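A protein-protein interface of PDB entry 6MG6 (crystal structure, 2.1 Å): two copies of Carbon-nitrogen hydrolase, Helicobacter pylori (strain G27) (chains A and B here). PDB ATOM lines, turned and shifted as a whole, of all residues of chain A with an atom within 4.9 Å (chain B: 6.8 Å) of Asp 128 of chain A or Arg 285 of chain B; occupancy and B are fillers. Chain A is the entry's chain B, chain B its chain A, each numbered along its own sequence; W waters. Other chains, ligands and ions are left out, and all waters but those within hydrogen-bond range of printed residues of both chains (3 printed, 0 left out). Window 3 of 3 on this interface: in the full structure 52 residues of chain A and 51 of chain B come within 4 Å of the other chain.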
ATOM      1  N   ILE A 126       9.621   5.646   6.276  1.00  0.00           N
ATOM      2  CA  ILE A 126      10.921   5.324   5.691  1.00  0.00           C
ATOM      3  C   ILE A 126      12.007   5.943   6.559  1.00  0.00           C
ATOM      4  O   ILE A 126      12.052   7.171   6.693  1.00  0.00           O
ATOM      5  CB  ILE A 126      11.030   5.838   4.250  1.00  0.00           C
ATOM      6  CG1 ILE A 126       9.796   5.422   3.434  1.00  0.00           C
ATOM      7  CG2 ILE A 126      12.287   5.263   3.612  1.00  0.00           C
ATOM      8  CD1 ILE A 126       9.646   3.926   3.300  1.00  0.00           C
ATOM      9  N   PRO A 127      12.930   5.159   7.116  1.00  0.00           N
ATOM     10  CA  PRO A 127      13.952   5.726   7.998  1.00  0.00           C
ATOM     11  C   PRO A 127      15.079   6.367   7.203  1.00  0.00           C
ATOM     12  O   PRO A 127      15.176   6.253   5.982  1.00  0.00           O
ATOM     13  CB  PRO A 127      14.453   4.520   8.793  1.00  0.00           C
ATOM     14  CG  PRO A 127      14.262   3.375   7.851  1.00  0.00           C
ATOM     15  CD  PRO A 127      13.013   3.691   7.050  1.00  0.00           C
ATOM     16  N   ASP A 128      15.923   7.086   7.932  1.00  0.00           N
ATOM     17  CA  ASP A 128      17.084   7.730   7.324  1.00  0.00           C
ATOM     18  C   ASP A 128      18.082   8.020   8.450  1.00  0.00           C
ATOM     19  O   ASP A 128      17.939   9.024   9.149  1.00  0.00           O
ATOM     20  CB  ASP A 128      16.684   9.003   6.580  1.00  0.00           C
ATOM     21  CG  ASP A 128      17.813   9.564   5.723  1.00  0.00           C
ATOM     22  OD1 ASP A 128      18.818   8.839   5.519  1.00  0.00           O
ATOM     23  OD2 ASP A 128      17.695  10.724   5.249  1.00  0.00           O
ATOM     24  N   ASP A 129      19.049   7.134   8.612  1.00  0.00           N
ATOM     25  CA  ASP A 129      20.173   7.312   9.530  1.00  0.00           C
ATOM     26  C   ASP A 129      21.412   6.769   8.858  1.00  0.00           C
ATOM     27  O   ASP A 129      21.327   5.973   7.918  1.00  0.00           O
ATOM     28  CB  ASP A 129      19.910   6.589  10.855  1.00  0.00           C
ATOM     29  CG  ASP A 129      20.447   7.343  12.019  1.00  0.00           C
ATOM     30  OD1 ASP A 129      19.861   8.386  12.357  1.00  0.00           O
ATOM     31  OD2 ASP A 129      21.476   6.921  12.573  1.00  0.00           O
ATOM     32  N   PRO A 130      22.615   7.185   9.299  1.00  0.00           N
ATOM     33  CA  PRO A 130      23.834   6.554   8.772  1.00  0.00           C
ATOM     34  C   PRO A 130      23.755   5.040   8.915  1.00  0.00           C
ATOM     35  O   PRO A 130      23.483   4.512   9.995  1.00  0.00           O
ATOM     36  CB  PRO A 130      24.947   7.154   9.638  1.00  0.00           C
ATOM     37  CG  PRO A 130      24.450   8.490   9.985  1.00  0.00           C
ATOM     38  CD  PRO A 130      22.949   8.326  10.176  1.00  0.00           C
ATOM     39  N   PHE A 132      21.433   3.315   7.466  1.00  0.00           N
ATOM     40  CA  PHE A 132      20.074   2.952   7.172  1.00  0.00           C
ATOM     41  C   PHE A 132      19.475   4.049   6.281  1.00  0.00           C
ATOM     42  O   PHE A 132      18.472   4.679   6.613  1.00  0.00           O
ATOM     43  CB  PHE A 132      19.310   2.732   8.477  1.00  0.00           C
ATOM     44  CG  PHE A 132      19.935   1.696   9.387  1.00  0.00           C
ATOM     45  CD1 PHE A 132      19.563   0.359   9.295  1.00  0.00           C
ATOM     46  CD2 PHE A 132      20.884   2.061  10.336  1.00  0.00           C
ATOM     47  CE1 PHE A 132      20.141  -0.601  10.123  1.00  0.00           C
ATOM     48  CE2 PHE A 132      21.471   1.108  11.178  1.00  0.00           C
ATOM     49  CZ  PHE A 132      21.090  -0.224  11.072  1.00  0.00           C
ATOM     50  N   TYR A 133      20.106   4.262   5.116  1.00  0.00           N
ATOM     51  CA  TYR A 133      19.747   5.345   4.192  1.00  0.00           C
ATOM     52  C   TYR A 133      18.548   4.965   3.324  1.00  0.00           C
ATOM     53  O   TYR A 133      18.589   5.017   2.094  1.00  0.00           O
ATOM     54  CB  TYR A 133      20.927   5.705   3.295  1.00  0.00           C
ATOM     55  CG  TYR A 133      22.172   6.201   3.990  1.00  0.00           C
ATOM     56  CD1 TYR A 133      22.267   7.523   4.433  1.00  0.00           C
ATOM     57  CD2 TYR A 133      23.275   5.367   4.160  1.00  0.00           C
ATOM     58  CE1 TYR A 133      23.421   7.989   5.051  1.00  0.00           C
ATOM     59  CE2 TYR A 133      24.435   5.825   4.786  1.00  0.00           C
ATOM     60  CZ  TYR A 133      24.494   7.134   5.229  1.00  0.00           C
ATOM     61  OH  TYR A 133      25.624   7.605   5.844  1.00  0.00           O
ATOM     62  N   GLU A 134      17.440   4.628   3.977  1.00  0.00           N
ATOM     63  CA  GLU A 134      16.324   4.082   3.210  1.00  0.00           C
ATOM     64  C   GLU A 134      15.589   5.147   2.414  1.00  0.00           C
ATOM     65  O   GLU A 134      15.053   4.834   1.339  1.00  0.00           O
ATOM     66  CB  GLU A 134      15.352   3.347   4.128  1.00  0.00           C
ATOM     67  CG  GLU A 134      15.992   2.109   4.741  1.00  0.00           C
ATOM     68  CD  GLU A 134      14.983   1.151   5.319  1.00  0.00           C
ATOM     69  OE1 GLU A 134      13.790   1.248   4.956  1.00  0.00           O
ATOM     70  OE2 GLU A 134      15.393   0.295   6.126  1.00  0.00           O
ATOM     71  N   LYS A 135      15.558   6.399   2.896  1.00  0.00           N
ATOM     72  CA  LYS A 135      14.826   7.450   2.178  1.00  0.00           C
ATOM     73  C   LYS A 135      15.421   7.733   0.797  1.00  0.00           C
ATOM     74  O   LYS A 135      14.708   8.222  -0.091  1.00  0.00           O
ATOM     75  CB  LYS A 135      14.782   8.759   2.993  1.00  0.00           C
ATOM     76  CG  LYS A 135      13.778   8.790   4.176  1.00  0.00           C
ATOM     77  CD  LYS A 135      13.767  10.218   4.809  1.00  0.00           C
ATOM     78  CE  LYS A 135      13.198  10.250   6.235  1.00  0.00           C
ATOM     79  NZ  LYS A 135      11.780   9.755   6.250  1.00  0.00           N
ATOM     80  N   ARG A 298       2.159  17.725  12.411  1.00  0.00           N
ATOM     81  CA  ARG A 298       3.562  17.383  12.564  1.00  0.00           C
ATOM     82  C   ARG A 298       4.037  17.733  13.961  1.00  0.00           C
ATOM     83  O   ARG A 298       4.835  17.006  14.553  1.00  0.00           O
ATOM     84  CB  ARG A 298       4.400  18.121  11.515  1.00  0.00           C
ATOM     85  CG  ARG A 298       5.944  17.907  11.668  1.00  0.00           C
ATOM     86  CD  ARG A 298       6.356  16.462  11.278  1.00  0.00           C
ATOM     87  NE  ARG A 298       5.891  16.106   9.932  1.00  0.00           N
ATOM     88  CZ  ARG A 298       5.769  14.859   9.487  1.00  0.00           C
ATOM     89  NH1 ARG A 298       6.105  13.839  10.267  1.00  0.00           N
ATOM     90  NH2 ARG A 298       5.330  14.626   8.258  1.00  0.00           N
ATOM     91  N   ARG B 279      17.206  12.496  18.273  1.00  0.00           N
ATOM     92  CA  ARG B 279      18.174  12.469  17.183  1.00  0.00           C
ATOM     93  C   ARG B 279      18.447  11.028  16.767  1.00  0.00           C
ATOM     94  O   ARG B 279      18.605  10.735  15.578  1.00  0.00           O
ATOM     95  CB  ARG B 279      19.484  13.158  17.591  1.00  0.00           C
ATOM     96  CG  ARG B 279      19.406  14.678  17.810  1.00  0.00           C
ATOM     97  CD  ARG B 279      20.786  15.272  18.142  1.00  0.00           C
ATOM     98  NE  ARG B 279      20.660  16.671  18.531  1.00  0.00           N
ATOM     99  CZ  ARG B 279      21.678  17.508  18.724  1.00  0.00           C
ATOM    100  NH1 ARG B 279      22.930  17.108  18.546  1.00  0.00           N
ATOM    101  NH2 ARG B 279      21.433  18.758  19.100  1.00  0.00           N
ATOM    102  N   TRP B 281      16.338   8.347  17.335  1.00  0.00           N
ATOM    103  CA  TRP B 281      15.089   7.724  16.912  1.00  0.00           C
ATOM    104  C   TRP B 281      14.137   8.841  16.500  1.00  0.00           C
ATOM    105  O   TRP B 281      13.289   9.281  17.296  1.00  0.00           O
ATOM    106  CB  TRP B 281      14.492   6.859  18.021  1.00  0.00           C
ATOM    107  CG  TRP B 281      15.100   5.464  18.114  1.00  0.00           C
ATOM    108  CD1 TRP B 281      15.802   4.802  17.145  1.00  0.00           C
ATOM    109  CD2 TRP B 281      15.029   4.570  19.232  1.00  0.00           C
ATOM    110  NE1 TRP B 281      16.189   3.559  17.595  1.00  0.00           N
ATOM    111  CE2 TRP B 281      15.726   3.390  18.872  1.00  0.00           C
ATOM    112  CE3 TRP B 281      14.441   4.651  20.503  1.00  0.00           C
ATOM    113  CZ2 TRP B 281      15.859   2.303  19.740  1.00  0.00           C
ATOM    114  CZ3 TRP B 281      14.577   3.573  21.368  1.00  0.00           C
ATOM    115  CH2 TRP B 281      15.283   2.414  20.981  1.00  0.00           C
ATOM    116  N   PRO B 282      14.255   9.335  15.267  1.00  0.00           N
ATOM    117  CA  PRO B 282      13.477  10.517  14.844  1.00  0.00           C
ATOM    118  C   PRO B 282      12.068  10.158  14.369  1.00  0.00           C
ATOM    119  O   PRO B 282      11.650  10.489  13.260  1.00  0.00           O
ATOM    120  CB  PRO B 282      14.355  11.097  13.727  1.00  0.00           C
ATOM    121  CG  PRO B 282      15.063   9.918  13.158  1.00  0.00           C
ATOM    122  CD  PRO B 282      15.293   8.957  14.287  1.00  0.00           C
ATOM    123  N   PHE B 283      11.303   9.514  15.252  1.00  0.00           N
ATOM    124  CA  PHE B 283       9.948   9.094  14.903  1.00  0.00           C
ATOM    125  C   PHE B 283       9.076  10.279  14.509  1.00  0.00           C
ATOM    126  O   PHE B 283       8.209  10.161  13.632  1.00  0.00           O
ATOM    127  CB  PHE B 283       9.315   8.339  16.074  1.00  0.00           C
ATOM    128  CG  PHE B 283      10.113   7.138  16.519  1.00  0.00           C
ATOM    129  CD1 PHE B 283      10.673   6.289  15.591  1.00  0.00           C
ATOM    130  CD2 PHE B 283      10.294   6.862  17.865  1.00  0.00           C
ATOM    131  CE1 PHE B 283      11.427   5.185  15.995  1.00  0.00           C
ATOM    132  CE2 PHE B 283      11.021   5.756  18.282  1.00  0.00           C
ATOM    133  CZ  PHE B 283      11.598   4.917  17.344  1.00  0.00           C
ATOM    134  N   LEU B 284       9.232  11.411  15.191  1.00  0.00           N
ATOM    135  CA  LEU B 284       8.343  12.526  14.897  1.00  0.00           C
ATOM    136  C   LEU B 284       8.576  13.066  13.487  1.00  0.00           C
ATOM    137  O   LEU B 284       7.633  13.511  12.825  1.00  0.00           O
ATOM    138  CB  LEU B 284       8.520  13.635  15.948  1.00  0.00           C
ATOM    139  CG  LEU B 284       8.155  13.282  17.399  1.00  0.00           C
ATOM    140  CD1 LEU B 284       8.332  14.531  18.274  1.00  0.00           C
ATOM    141  CD2 LEU B 284       6.707  12.758  17.511  1.00  0.00           C
ATOM    142  N   ARG B 285       9.832  13.055  13.025  1.00  0.00           N
ATOM    143  CA  ARG B 285      10.154  13.494  11.671  1.00  0.00           C
ATOM    144  C   ARG B 285       9.464  12.630  10.626  1.00  0.00           C
ATOM    145  O   ARG B 285       9.083  13.125   9.556  1.00  0.00           O
ATOM    146  CB  ARG B 285      11.671  13.430  11.449  1.00  0.00           C
ATOM    147  CG  ARG B 285      12.146  13.870  10.051  1.00  0.00           C
ATOM    148  CD  ARG B 285      13.622  13.456   9.777  1.00  0.00           C
ATOM    149  NE  ARG B 285      13.728  12.005   9.740  1.00  0.00           N
ATOM    150  CZ  ARG B 285      14.859  11.308   9.802  1.00  0.00           C
ATOM    151  NH1 ARG B 285      16.023  11.913   9.917  1.00  0.00           N
ATOM    152  NH2 ARG B 285      14.809   9.987   9.770  1.00  0.00           N
ATOM    153  N   ASP B 286       9.309  11.341  10.902  1.00  0.00           N
ATOM    154  CA  ASP B 286       8.893  10.391   9.882  1.00  0.00           C
ATOM    155  C   ASP B 286       7.421  10.010   9.962  1.00  0.00           C
ATOM    156  O   ASP B 286       6.945   9.293   9.081  1.00  0.00           O
ATOM    157  CB  ASP B 286       9.747   9.116   9.968  1.00  0.00           C
ATOM    158  CG  ASP B 286      11.193   9.367   9.619  1.00  0.00           C
ATOM    159  OD1 ASP B 286      11.442  10.371   8.927  1.00  0.00           O
ATOM    160  OD2 ASP B 286      12.074   8.571  10.010  1.00  0.00           O
ATOM    161  N   ARG B 287       6.683  10.489  10.962  1.00  0.00           N
ATOM    162  CA  ARG B 287       5.266  10.146  11.060  1.00  0.00           C
ATOM    163  C   ARG B 287       4.561  10.469   9.751  1.00  0.00           C
ATOM    164  O   ARG B 287       4.776  11.532   9.176  1.00  0.00           O
ATOM    165  CB  ARG B 287       4.611  10.901  12.224  1.00  0.00           C
ATOM    166  CG  ARG B 287       4.966  10.341  13.580  1.00  0.00           C
ATOM    167  CD  ARG B 287       4.375  11.197  14.701  1.00  0.00           C
ATOM    168  NE  ARG B 287       2.924  11.054  14.819  1.00  0.00           N
ATOM    169  CZ  ARG B 287       2.051  12.041  14.600  1.00  0.00           C
ATOM    170  NH1 ARG B 287       2.489  13.255  14.263  1.00  0.00           N
ATOM    171  NH2 ARG B 287       0.734  11.824  14.746  1.00  0.00           N
ATOM    172  N   ARG B 288       3.759   9.527   9.250  1.00  0.00           N
ATOM    173  CA  ARG B 288       3.042   9.731   7.982  1.00  0.00           C
ATOM    174  C   ARG B 288       1.680  10.380   8.247  1.00  0.00           C
ATOM    175  O   ARG B 288       0.616   9.813   7.993  1.00  0.00           O
ATOM    176  CB  ARG B 288       2.892   8.407   7.229  1.00  0.00           C
ATOM    177  CG  ARG B 288       4.208   7.845   6.610  1.00  0.00           C
ATOM    178  CD  ARG B 288       4.802   8.791   5.521  1.00  0.00           C
ATOM    179  NE  ARG B 288       3.835   9.114   4.455  1.00  0.00           N
ATOM    180  CZ  ARG B 288       3.545   8.324   3.410  1.00  0.00           C
ATOM    181  NH1 ARG B 288       4.125   7.133   3.256  1.00  0.00           N
ATOM    182  NH2 ARG B 288       2.667   8.725   2.497  1.00  0.00           N
HETATM  183  O   HOH W   1       5.149  14.440  13.946  1.00  0.00           O
HETATM  184  O   HOH W   2       8.554   8.486   6.816  1.00  0.00           O
HETATM  185  O   HOH W   3      15.610   7.245  10.779  1.00  0.00           O
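NE of Arg 285 of chain B is in salt-bridge range of OD1 of Asp 286 of chain B, 2.9 Å away. The side-chain amino group (NZ) of Lys 135 of chain A lies within hydrogen-bond range of the backbone carbonyl oxygen (O) of Ile 126 of chain A, 2.6 Å away. The backbone NH (N) of Glu 134 of chain A lies within hydrogen-bond range of the backbone carbonyl oxygen (O) of Pro 127 of chain A (3.4 Å). The backbone NH (N) of Lys 135 of chain A sits at hydrogen-bond distance from the backbone carbonyl oxygen (O) of Pro 127 of chain A (3.1 Å).
Among the printed residues, pairs that only touch across the chains: Ile 126 of chain A with Asp 286 of chain B (3.6 Å), Pro 127 of chain A with Asp 286 of chain B (3.96 Å) and Lys 135 of chain A with Arg 285 of chain B (3.9 Å).
Along chain A the printed residues that touch a printed residue of chain B span positions 126 to 298. Printed residues of chain B that touch a printed residue of chain A: Leu 284, Arg 285, Asp 286 and Arg 287. Among the printed residues, 8 pairs touch across the chains.
No position is printed for both chains.
Water W1 lies within hydrogen-bond range of the backbone carbonyl oxygen of Arg 298 of chain A (2.7 Å), the backbone carbonyl oxygen of Leu 284 of chain B (2.9 Å) and the guanidinium group of Arg 287 of chain B (2.9 Å). Water W3 lies within hydrogen-bond range of N of Asp 128 of chain A (2.9 Å) and NH2 of Arg 285 of chain B (3.0 Å). Water W2 bridges O of Asp 286 of chain B and N of Ile 126 of chain A.
Asp 128 of chain A touches just one residue of chain B: Arg 285. Of chain A, only Asp 128, Lys 135 and Arg 298 come within 4 Å of Arg 285 of chain B. Of the printed residues of chain B, Lys 135 of chain A touches Arg 285 and Asp 286. Of the printed residues of chain B, Ile 126 of chain A touches Asp 286 (3.6 Å). Of the printed residues of chain A, Arg 287 of chain B touches Arg 298 (2.9 Å). Arg 279 of chain B touches none of the printed residues of chain A. The nearest residue of chain B that does not touch Asp 128 of chain A is Asp 286 of chain B (4.6 Å). The nearest printed residue of chain B that does not touch Arg 298 of chain A is Asp 286 of chain B (4.1 Å).
O of Leu 284 of chain B lies within hydrogen-bond range of NH1 of Arg 298 of chain A (3.0 Å). NH2 of Arg 285 of chain B sits at hydrogen-bond distance from O of Asp 128 of chain A, 3.3 Å away. NH1 of Arg 298 of chain A is in hydrogen-bond range of O of Arg 285 of chain B (3.1 Å). NZ of Lys 135 of chain A is in salt-bridge range of OD1 of Asp 286 of chain B (2.8 Å). O of Arg 287 of chain B lies within hydrogen-bond range of NH1 of Arg 298 of chain A (2.9 Å).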
